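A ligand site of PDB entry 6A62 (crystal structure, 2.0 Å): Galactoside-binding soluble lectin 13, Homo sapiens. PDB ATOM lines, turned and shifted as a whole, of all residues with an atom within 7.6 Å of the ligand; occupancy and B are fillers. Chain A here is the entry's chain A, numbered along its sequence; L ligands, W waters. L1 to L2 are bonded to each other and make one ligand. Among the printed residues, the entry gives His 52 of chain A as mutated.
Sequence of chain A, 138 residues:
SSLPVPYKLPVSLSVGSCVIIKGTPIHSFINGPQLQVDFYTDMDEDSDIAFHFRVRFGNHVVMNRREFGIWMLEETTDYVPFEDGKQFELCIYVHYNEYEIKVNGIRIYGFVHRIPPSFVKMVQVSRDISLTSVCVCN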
ATOM      1  N   GLN A  34       0.681  -8.515   0.105  1.00  0.00           N
ATOM      2  CA  GLN A  34       1.431  -7.450  -0.561  1.00  0.00           C
ATOM      3  C   GLN A  34       2.750  -7.221   0.144  1.00  0.00           C
ATOM      4  O   GLN A  34       2.910  -7.544   1.327  1.00  0.00           O
ATOM      5  CB  GLN A  34       0.639  -6.131  -0.603  1.00  0.00           C
ATOM      6  CG  GLN A  34      -0.599  -6.187  -1.499  1.00  0.00           C
ATOM      7  CD  GLN A  34      -1.504  -4.974  -1.376  1.00  0.00           C
ATOM      8  OE1 GLN A  34      -2.662  -5.012  -1.775  1.00  0.00           O
ATOM      9  NE2 GLN A  34      -0.984  -3.900  -0.804  1.00  0.00           N
ATOM     10  N   GLN A  36       5.626  -3.889   0.283  1.00  0.00           N
ATOM     11  CA  GLN A  36       5.848  -2.500  -0.118  1.00  0.00           C
ATOM     12  C   GLN A  36       7.239  -2.032   0.313  1.00  0.00           C
ATOM     13  O   GLN A  36       7.631  -2.236   1.470  1.00  0.00           O
ATOM     14  CB  GLN A  36       4.788  -1.561   0.467  1.00  0.00           C
ATOM     15  CG  GLN A  36       4.836  -0.165  -0.167  1.00  0.00           C
ATOM     16  CD  GLN A  36       3.652   0.704   0.191  1.00  0.00           C
ATOM     17  OE1 GLN A  36       2.492   0.319   0.041  1.00  0.00           O
ATOM     18  NE2 GLN A  36       3.959   1.899   0.721  1.00  0.00           N
ATOM     19  N   ASP A  38       9.435   1.630   0.170  1.00  0.00           N
ATOM     20  CA  ASP A  38       9.437   3.060  -0.130  1.00  0.00           C
ATOM     21  C   ASP A  38      10.832   3.623   0.107  1.00  0.00           C
ATOM     22  O   ASP A  38      11.418   3.392   1.166  1.00  0.00           O
ATOM     23  CB  ASP A  38       8.434   3.831   0.718  1.00  0.00           C
ATOM     24  CG  ASP A  38       6.994   3.446   0.429  1.00  0.00           C
ATOM     25  OD1 ASP A  38       6.468   3.813  -0.650  1.00  0.00           O
ATOM     26  OD2 ASP A  38       6.373   2.781   1.294  1.00  0.00           O
ATOM     27  N   ILE A  49       8.654  10.762  -1.674  1.00  0.00           N
ATOM     28  CA  ILE A  49       9.125   9.403  -1.908  1.00  0.00           C
ATOM     29  C   ILE A  49       9.759   9.358  -3.288  1.00  0.00           C
ATOM     30  O   ILE A  49       9.081   9.596  -4.291  1.00  0.00           O
ATOM     31  CB  ILE A  49       7.976   8.387  -1.810  1.00  0.00           C
ATOM     32  CG1 ILE A  49       7.396   8.386  -0.387  1.00  0.00           C
ATOM     33  CG2 ILE A  49       8.434   6.970  -2.208  1.00  0.00           C
ATOM     34  CD1 ILE A  49       6.089   7.591  -0.278  1.00  0.00           C
ATOM     35  N   HIS A  52       8.594   4.302  -4.969  1.00  0.00           N
ATOM     36  CA  HIS A  52       7.588   3.517  -4.266  1.00  0.00           C
ATOM     37  C   HIS A  52       7.347   2.254  -5.079  1.00  0.00           C
ATOM     38  O   HIS A  52       7.120   2.329  -6.297  1.00  0.00           O
ATOM     39  CB  HIS A  52       6.304   4.344  -4.107  1.00  0.00           C
ATOM     40  CG  HIS A  52       5.073   3.530  -3.824  1.00  0.00           C
ATOM     41  ND1 HIS A  52       4.740   3.095  -2.558  1.00  0.00           N
ATOM     42  CD2 HIS A  52       4.068   3.140  -4.634  1.00  0.00           C
ATOM     43  CE1 HIS A  52       3.596   2.436  -2.608  1.00  0.00           C
ATOM     44  NE2 HIS A  52       3.161   2.457  -3.853  1.00  0.00           N
ATOM     45  N   PHE A  53       7.427   1.112  -4.426  1.00  0.00           N
ATOM     46  CA  PHE A  53       7.368  -0.199  -5.076  1.00  0.00           C
ATOM     47  C   PHE A  53       6.399  -1.058  -4.283  1.00  0.00           C
ATOM     48  O   PHE A  53       6.614  -1.307  -3.098  1.00  0.00           O
ATOM     49  CB  PHE A  53       8.775  -0.797  -5.105  1.00  0.00           C
ATOM     50  CG  PHE A  53       8.850  -2.218  -5.595  1.00  0.00           C
ATOM     51  CD1 PHE A  53       8.967  -2.503  -6.943  1.00  0.00           C
ATOM     52  CD2 PHE A  53       8.912  -3.273  -4.688  1.00  0.00           C
ATOM     53  CE1 PHE A  53       9.077  -3.803  -7.388  1.00  0.00           C
ATOM     54  CE2 PHE A  53       9.025  -4.575  -5.124  1.00  0.00           C
ATOM     55  CZ  PHE A  53       9.113  -4.843  -6.477  1.00  0.00           C
ATOM     56  N   ARG A  54       5.308  -1.480  -4.913  1.00  0.00           N
ATOM     57  CA  ARG A  54       4.252  -2.195  -4.193  1.00  0.00           C
ATOM     58  C   ARG A  54       3.852  -3.446  -4.974  1.00  0.00           C
ATOM     59  O   ARG A  54       3.217  -3.357  -6.019  1.00  0.00           O
ATOM     60  CB  ARG A  54       3.049  -1.281  -3.986  1.00  0.00           C
ATOM     61  CG  ARG A  54       1.950  -1.900  -3.157  1.00  0.00           C
ATOM     62  CD  ARG A  54       1.129  -0.781  -2.587  1.00  0.00           C
ATOM     63  NE  ARG A  54      -0.157  -1.221  -2.137  1.00  0.00           N
ATOM     64  CZ  ARG A  54      -1.088  -0.409  -1.641  1.00  0.00           C
ATOM     65  NH1 ARG A  54      -0.845   0.892  -1.553  1.00  0.00           N
ATOM     66  NH2 ARG A  54      -2.257  -0.901  -1.223  1.00  0.00           N
ATOM     67  N   HIS A  60       0.416  -8.180  -9.754  1.00  0.00           N
ATOM     68  CA  HIS A  60       1.182  -7.177 -10.487  1.00  0.00           C
ATOM     69  C   HIS A  60       1.961  -6.322  -9.500  1.00  0.00           C
ATOM     70  O   HIS A  60       1.832  -6.469  -8.277  1.00  0.00           O
ATOM     71  CB  HIS A  60       0.267  -6.308 -11.373  1.00  0.00           C
ATOM     72  CG  HIS A  60      -0.654  -5.424 -10.594  1.00  0.00           C
ATOM     73  ND1 HIS A  60      -1.929  -5.800 -10.237  1.00  0.00           N
ATOM     74  CD2 HIS A  60      -0.486  -4.174 -10.088  1.00  0.00           C
ATOM     75  CE1 HIS A  60      -2.502  -4.827  -9.557  1.00  0.00           C
ATOM     76  NE2 HIS A  60      -1.649  -3.827  -9.452  1.00  0.00           N
ATOM     77  N   VAL A  62       2.994  -2.241  -8.664  1.00  0.00           N
ATOM     78  CA  VAL A  62       2.768  -0.815  -8.891  1.00  0.00           C
ATOM     79  C   VAL A  62       3.978  -0.035  -8.406  1.00  0.00           C
ATOM     80  O   VAL A  62       4.498  -0.292  -7.310  1.00  0.00           O
ATOM     81  CB  VAL A  62       1.478  -0.342  -8.190  1.00  0.00           C
ATOM     82  CG1 VAL A  62       1.460   1.167  -8.079  1.00  0.00           C
ATOM     83  CG2 VAL A  62       0.260  -0.844  -8.947  1.00  0.00           C
ATOM     84  N   MET A  63       4.437   0.912  -9.221  1.00  0.00           N
ATOM     85  CA  MET A  63       5.578   1.766  -8.879  1.00  0.00           C
ATOM     86  C   MET A  63       5.216   3.221  -9.114  1.00  0.00           C
ATOM     87  O   MET A  63       4.490   3.546 -10.053  1.00  0.00           O
ATOM     88  CB  MET A  63       6.813   1.402  -9.688  1.00  0.00           C
ATOM     89  CG  MET A  63       7.466   0.133  -9.220  1.00  0.00           C
ATOM     90  SD  MET A  63       8.488  -0.571 -10.502  1.00  0.00           S
ATOM     91  CE  MET A  63       7.202  -0.812 -11.755  1.00  0.00           C
ATOM     92  N   ASN A  64       5.727   4.109  -8.264  1.00  0.00           N
ATOM     93  CA  ASN A  64       5.427   5.524  -8.403  1.00  0.00           C
ATOM     94  C   ASN A  64       6.433   6.330  -7.591  1.00  0.00           C
ATOM     95  O   ASN A  64       7.339   5.781  -6.945  1.00  0.00           O
ATOM     96  CB  ASN A  64       3.996   5.845  -7.951  1.00  0.00           C
ATOM     97  CG  ASN A  64       3.379   7.049  -8.665  1.00  0.00           C
ATOM     98  OD1 ASN A  64       4.062   7.817  -9.344  1.00  0.00           O
ATOM     99  ND2 ASN A  64       2.064   7.216  -8.528  1.00  0.00           N
ATOM    100  N   ARG A  65       6.247   7.636  -7.616  1.00  0.00           N
ATOM    101  CA  ARG A  65       6.937   8.499  -6.675  1.00  0.00           C
ATOM    102  C   ARG A  65       5.939   9.544  -6.185  1.00  0.00           C
ATOM    103  O   ARG A  65       4.871   9.732  -6.768  1.00  0.00           O
ATOM    104  CB  ARG A  65       8.177   9.143  -7.328  1.00  0.00           C
ATOM    105  CG  ARG A  65       7.821  10.117  -8.363  1.00  0.00           C
ATOM    106  CD  ARG A  65       8.378   9.774  -9.728  1.00  0.00           C
ATOM    107  NE  ARG A  65       8.239  10.967 -10.546  1.00  0.00           N
ATOM    108  CZ  ARG A  65       7.523  11.083 -11.660  1.00  0.00           C
ATOM    109  NH1 ARG A  65       6.872  10.046 -12.162  1.00  0.00           N
ATOM    110  NH2 ARG A  65       7.484  12.261 -12.268  1.00  0.00           N
ATOM    111  N   ARG A  66       6.284  10.189  -5.075  1.00  0.00           N
ATOM    112  CA  ARG A  66       5.453  11.225  -4.485  1.00  0.00           C
ATOM    113  C   ARG A  66       6.286  12.498  -4.377  1.00  0.00           C
ATOM    114  O   ARG A  66       7.293  12.523  -3.661  1.00  0.00           O
ATOM    115  CB  ARG A  66       4.942  10.815  -3.108  1.00  0.00           C
ATOM    116  CG  ARG A  66       3.846  11.723  -2.580  1.00  0.00           C
ATOM    117  CD  ARG A  66       3.104  11.068  -1.419  1.00  0.00           C
ATOM    118  NE  ARG A  66       3.916  11.016  -0.212  1.00  0.00           N
ATOM    119  CZ  ARG A  66       3.703  10.164   0.791  1.00  0.00           C
ATOM    120  NH1 ARG A  66       2.702   9.283   0.692  1.00  0.00           N
ATOM    121  NH2 ARG A  66       4.484  10.172   1.858  1.00  0.00           N
ATOM    122  N   TRP A  71       1.042  12.114  -5.526  1.00  0.00           N
ATOM    123  CA  TRP A  71       1.469  10.951  -6.304  1.00  0.00           C
ATOM    124  C   TRP A  71       1.538  11.308  -7.789  1.00  0.00           C
ATOM    125  O   TRP A  71       0.684  12.020  -8.311  1.00  0.00           O
ATOM    126  CB  TRP A  71       0.522   9.784  -6.075  1.00  0.00           C
ATOM    127  CG  TRP A  71       0.624   9.193  -4.688  1.00  0.00           C
ATOM    128  CD1 TRP A  71      -0.254   9.362  -3.651  1.00  0.00           C
ATOM    129  CD2 TRP A  71       1.640   8.320  -4.201  1.00  0.00           C
ATOM    130  NE1 TRP A  71       0.164   8.658  -2.551  1.00  0.00           N
ATOM    131  CE2 TRP A  71       1.322   8.002  -2.859  1.00  0.00           C
ATOM    132  CE3 TRP A  71       2.797   7.768  -4.767  1.00  0.00           C
ATOM    133  CZ2 TRP A  71       2.117   7.165  -2.079  1.00  0.00           C
ATOM    134  CZ3 TRP A  71       3.590   6.940  -3.984  1.00  0.00           C
ATOM    135  CH2 TRP A  71       3.246   6.643  -2.660  1.00  0.00           C
ATOM    136  N   MET A  72       2.566  10.808  -8.465  1.00  0.00           N
ATOM    137  CA  MET A  72       2.803  11.129  -9.868  1.00  0.00           C
ATOM    138  C   MET A  72       2.231  10.029 -10.760  1.00  0.00           C
ATOM    139  O   MET A  72       1.325   9.280 -10.344  1.00  0.00           O
ATOM    140  CB  MET A  72       4.315  11.360 -10.089  1.00  0.00           C
ATOM    141  CG  MET A  72       4.926  12.453  -9.217  1.00  0.00           C
ATOM    142  SD  MET A  72       4.108  14.066  -9.395  1.00  0.00           S
ATOM    143  CE  MET A  72       4.986  14.688 -10.807  1.00  0.00           C
ATOM    144  N   LEU A  73       2.745   9.898 -11.978  1.00  0.00           N
ATOM    145  CA  LEU A  73       2.184   8.944 -12.921  1.00  0.00           C
ATOM    146  C   LEU A  73       2.592   7.527 -12.541  1.00  0.00           C
ATOM    147  O   LEU A  73       3.787   7.192 -12.524  1.00  0.00           O
ATOM    148  CB  LEU A  73       2.626   9.253 -14.357  1.00  0.00           C
ATOM    149  CG  LEU A  73       1.705   8.551 -15.378  1.00  0.00           C
ATOM    150  CD1 LEU A  73       0.234   8.880 -15.108  1.00  0.00           C
ATOM    151  CD2 LEU A  73       2.055   8.913 -16.803  1.00  0.00           C
ATOM    152  N   GLU A  74       1.610   6.684 -12.279  1.00  0.00           N
ATOM    153  CA  GLU A  74       1.854   5.323 -11.842  1.00  0.00           C
ATOM    154  C   GLU A  74       2.478   4.496 -12.953  1.00  0.00           C
ATOM    155  O   GLU A  74       2.072   4.570 -14.110  1.00  0.00           O
ATOM    156  CB  GLU A  74       0.537   4.704 -11.418  1.00  0.00           C
ATOM    157  CG  GLU A  74       0.594   3.836 -10.230  1.00  0.00           C
ATOM    158  CD  GLU A  74      -0.799   3.508  -9.761  1.00  0.00           C
ATOM    159  OE1 GLU A  74      -1.207   4.028  -8.696  1.00  0.00           O
ATOM    160  OE2 GLU A  74      -1.500   2.767 -10.488  1.00  0.00           O
ATOM    161  N   GLU A  75       3.467   3.682 -12.597  1.00  0.00           N
ATOM    162  CA  GLU A  75       4.060   2.696 -13.493  1.00  0.00           C
ATOM    163  C   GLU A  75       3.749   1.298 -12.983  1.00  0.00           C
ATOM    164  O   GLU A  75       3.548   1.101 -11.783  1.00  0.00           O
ATOM    165  CB  GLU A  75       5.571   2.915 -13.613  1.00  0.00           C
ATOM    166  CG  GLU A  75       5.921   4.352 -14.019  1.00  0.00           C
ATOM    167  CD  GLU A  75       7.425   4.635 -14.077  1.00  0.00           C
ATOM    168  OE1 GLU A  75       8.191   3.750 -14.512  1.00  0.00           O
ATOM    169  OE2 GLU A  75       7.821   5.756 -13.695  1.00  0.00           O
ATOM    170  N   ARG A 127       4.063  -4.064   4.972  1.00  0.00           N
ATOM    171  CA  ARG A 127       2.911  -4.918   4.657  1.00  0.00           C
ATOM    172  C   ARG A 127       3.141  -6.389   4.996  1.00  0.00           C
ATOM    173  O   ARG A 127       3.706  -6.707   6.046  1.00  0.00           O
ATOM    174  CB  ARG A 127       2.478  -4.703   3.206  1.00  0.00           C
ATOM    175  CG  ARG A 127       2.066  -3.250   3.015  1.00  0.00           C
ATOM    176  CD  ARG A 127       1.156  -3.017   1.849  1.00  0.00           C
ATOM    177  NE  ARG A 127       1.059  -1.586   1.585  1.00  0.00           N
ATOM    178  CZ  ARG A 127       0.019  -0.826   1.906  1.00  0.00           C
ATOM    179  NH1 ARG A 127       0.051   0.474   1.631  1.00  0.00           N
ATOM    180  NH2 ARG A 127      -1.058  -1.354   2.497  1.00  0.00           N
HETATM  181  C1  LIG L   1      -4.986   4.162  -8.140  1.00  0.00           C
HETATM  182  C2  LIG L   1      -4.397   3.669  -6.893  1.00  0.00           C
HETATM  183  C3  LIG L   1      -3.935   4.747  -6.068  1.00  0.00           C
HETATM  184  C4  LIG L   1      -5.034   5.711  -5.785  1.00  0.00           C
HETATM  185  C5  LIG L   1      -4.551   6.885  -4.914  1.00  0.00           C
HETATM  186  C6  LIG L   1      -6.197   5.053  -7.833  1.00  0.00           C
HETATM  187  O1  LIG L   1      -6.706   5.498  -8.948  1.00  0.00           O
HETATM  188  O2  LIG L   1      -5.413   3.032  -8.949  1.00  0.00           O
HETATM  189  O3  LIG L   1      -3.268   2.735  -7.217  1.00  0.00           O
HETATM  190  O4  LIG L   1      -3.500   4.141  -4.762  1.00  0.00           O
HETATM  191  O5  LIG L   1      -5.667   6.206  -7.000  1.00  0.00           O
HETATM  192  O6  LIG L   1      -3.975   7.864  -5.721  1.00  0.00           O
HETATM  193  C1  LG2 L   2      -2.341   4.718  -4.343  1.00  0.00           C
HETATM  194  C2  LG2 L   2      -2.014   4.169  -2.951  1.00  0.00           C
HETATM  195  C3  LG2 L   2      -0.631   4.529  -2.517  1.00  0.00           C
HETATM  196  C4  LG2 L   2       0.380   4.186  -3.532  1.00  0.00           C
HETATM  197  C5  LG2 L   2       0.052   4.844  -4.866  1.00  0.00           C
HETATM  198  C6  LG2 L   2       1.031   4.414  -5.862  1.00  0.00           C
HETATM  199  O1  LG2 L   2      -2.935   4.701  -2.037  1.00  0.00           O
HETATM  200  O2  LG2 L   2      -0.344   3.825  -1.265  1.00  0.00           O
HETATM  201  O3  LG2 L   2       0.380   2.748  -3.743  1.00  0.00           O
HETATM  202  O4  LG2 L   2      -1.319   4.435  -5.339  1.00  0.00           O
HETATM  203  O5  LG2 L   2       0.719   5.020  -7.057  1.00  0.00           O
HETATM  204  O   HOH W   1      -1.535   7.340  -7.359  1.00  0.00           O
HETATM  205  O   HOH W   2       1.962   3.691   0.157  1.00  0.00           O
HETATM  206  O   HOH W   3      -2.793   7.115  -1.382  1.00  0.00           O
HETATM  207  O   HOH W   4      -1.583   0.827  -5.269  1.00  0.00           O
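The side-chain carboxylate of Glu 74 lies within hydrogen-bond range of an oxygen (O5) of LG2 L2 (2.7 Å).
O5 of LG2 L2 is in hydrogen-bond range of ND2 of Asn 64 (3.0 Å).
The guanidinium group (NH1) of Arg 54 is in hydrogen-bond range of an oxygen (O2) of LG2 L2, 3.0 Å away.
An oxygen (O3) of LG2 L2 sits at hydrogen-bond distance from a ring nitrogen (NE2) of His 52 (2.8 Å).
OD1 of Asp 38 sits at hydrogen-bond distance from ND1 of His 52, at 2.7 Å.
The side-chain amide oxygen (OD1) of Asn 64 sits close to the backbone carbonyl oxygen (O) of Leu 73, 3.3 Å away.
The backbone carbonyl oxygen of Met 72 sits at hydrogen-bond distance from the side-chain amide nitrogen of Asn 64, at 2.8 Å.
The backbone NH of His 52 is in hydrogen-bond range of the backbone carbonyl oxygen of Asn 64 (2.8 Å).
N of Arg 54 lies within hydrogen-bond range of O of Val 62 (2.8 Å).
The guanidinium group of Arg 54 sits close to the side-chain amide nitrogen of Gln 34.
Residues that only touch the ligand: Trp 71 (3.7 Å) and Val 62 (3.96 Å).
Hydrophobic or aromatic side chains within 4 Å of the ligand: His 52, Val 62 and Trp 71.
Within 4 Å of the ligand: His 52, Arg 54, Val 62, Asn 64, Trp 71 and Glu 74.
Water W2 bridges an oxygen (O2) of LG2 L2 and the side-chain amide nitrogen of Gln 36.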
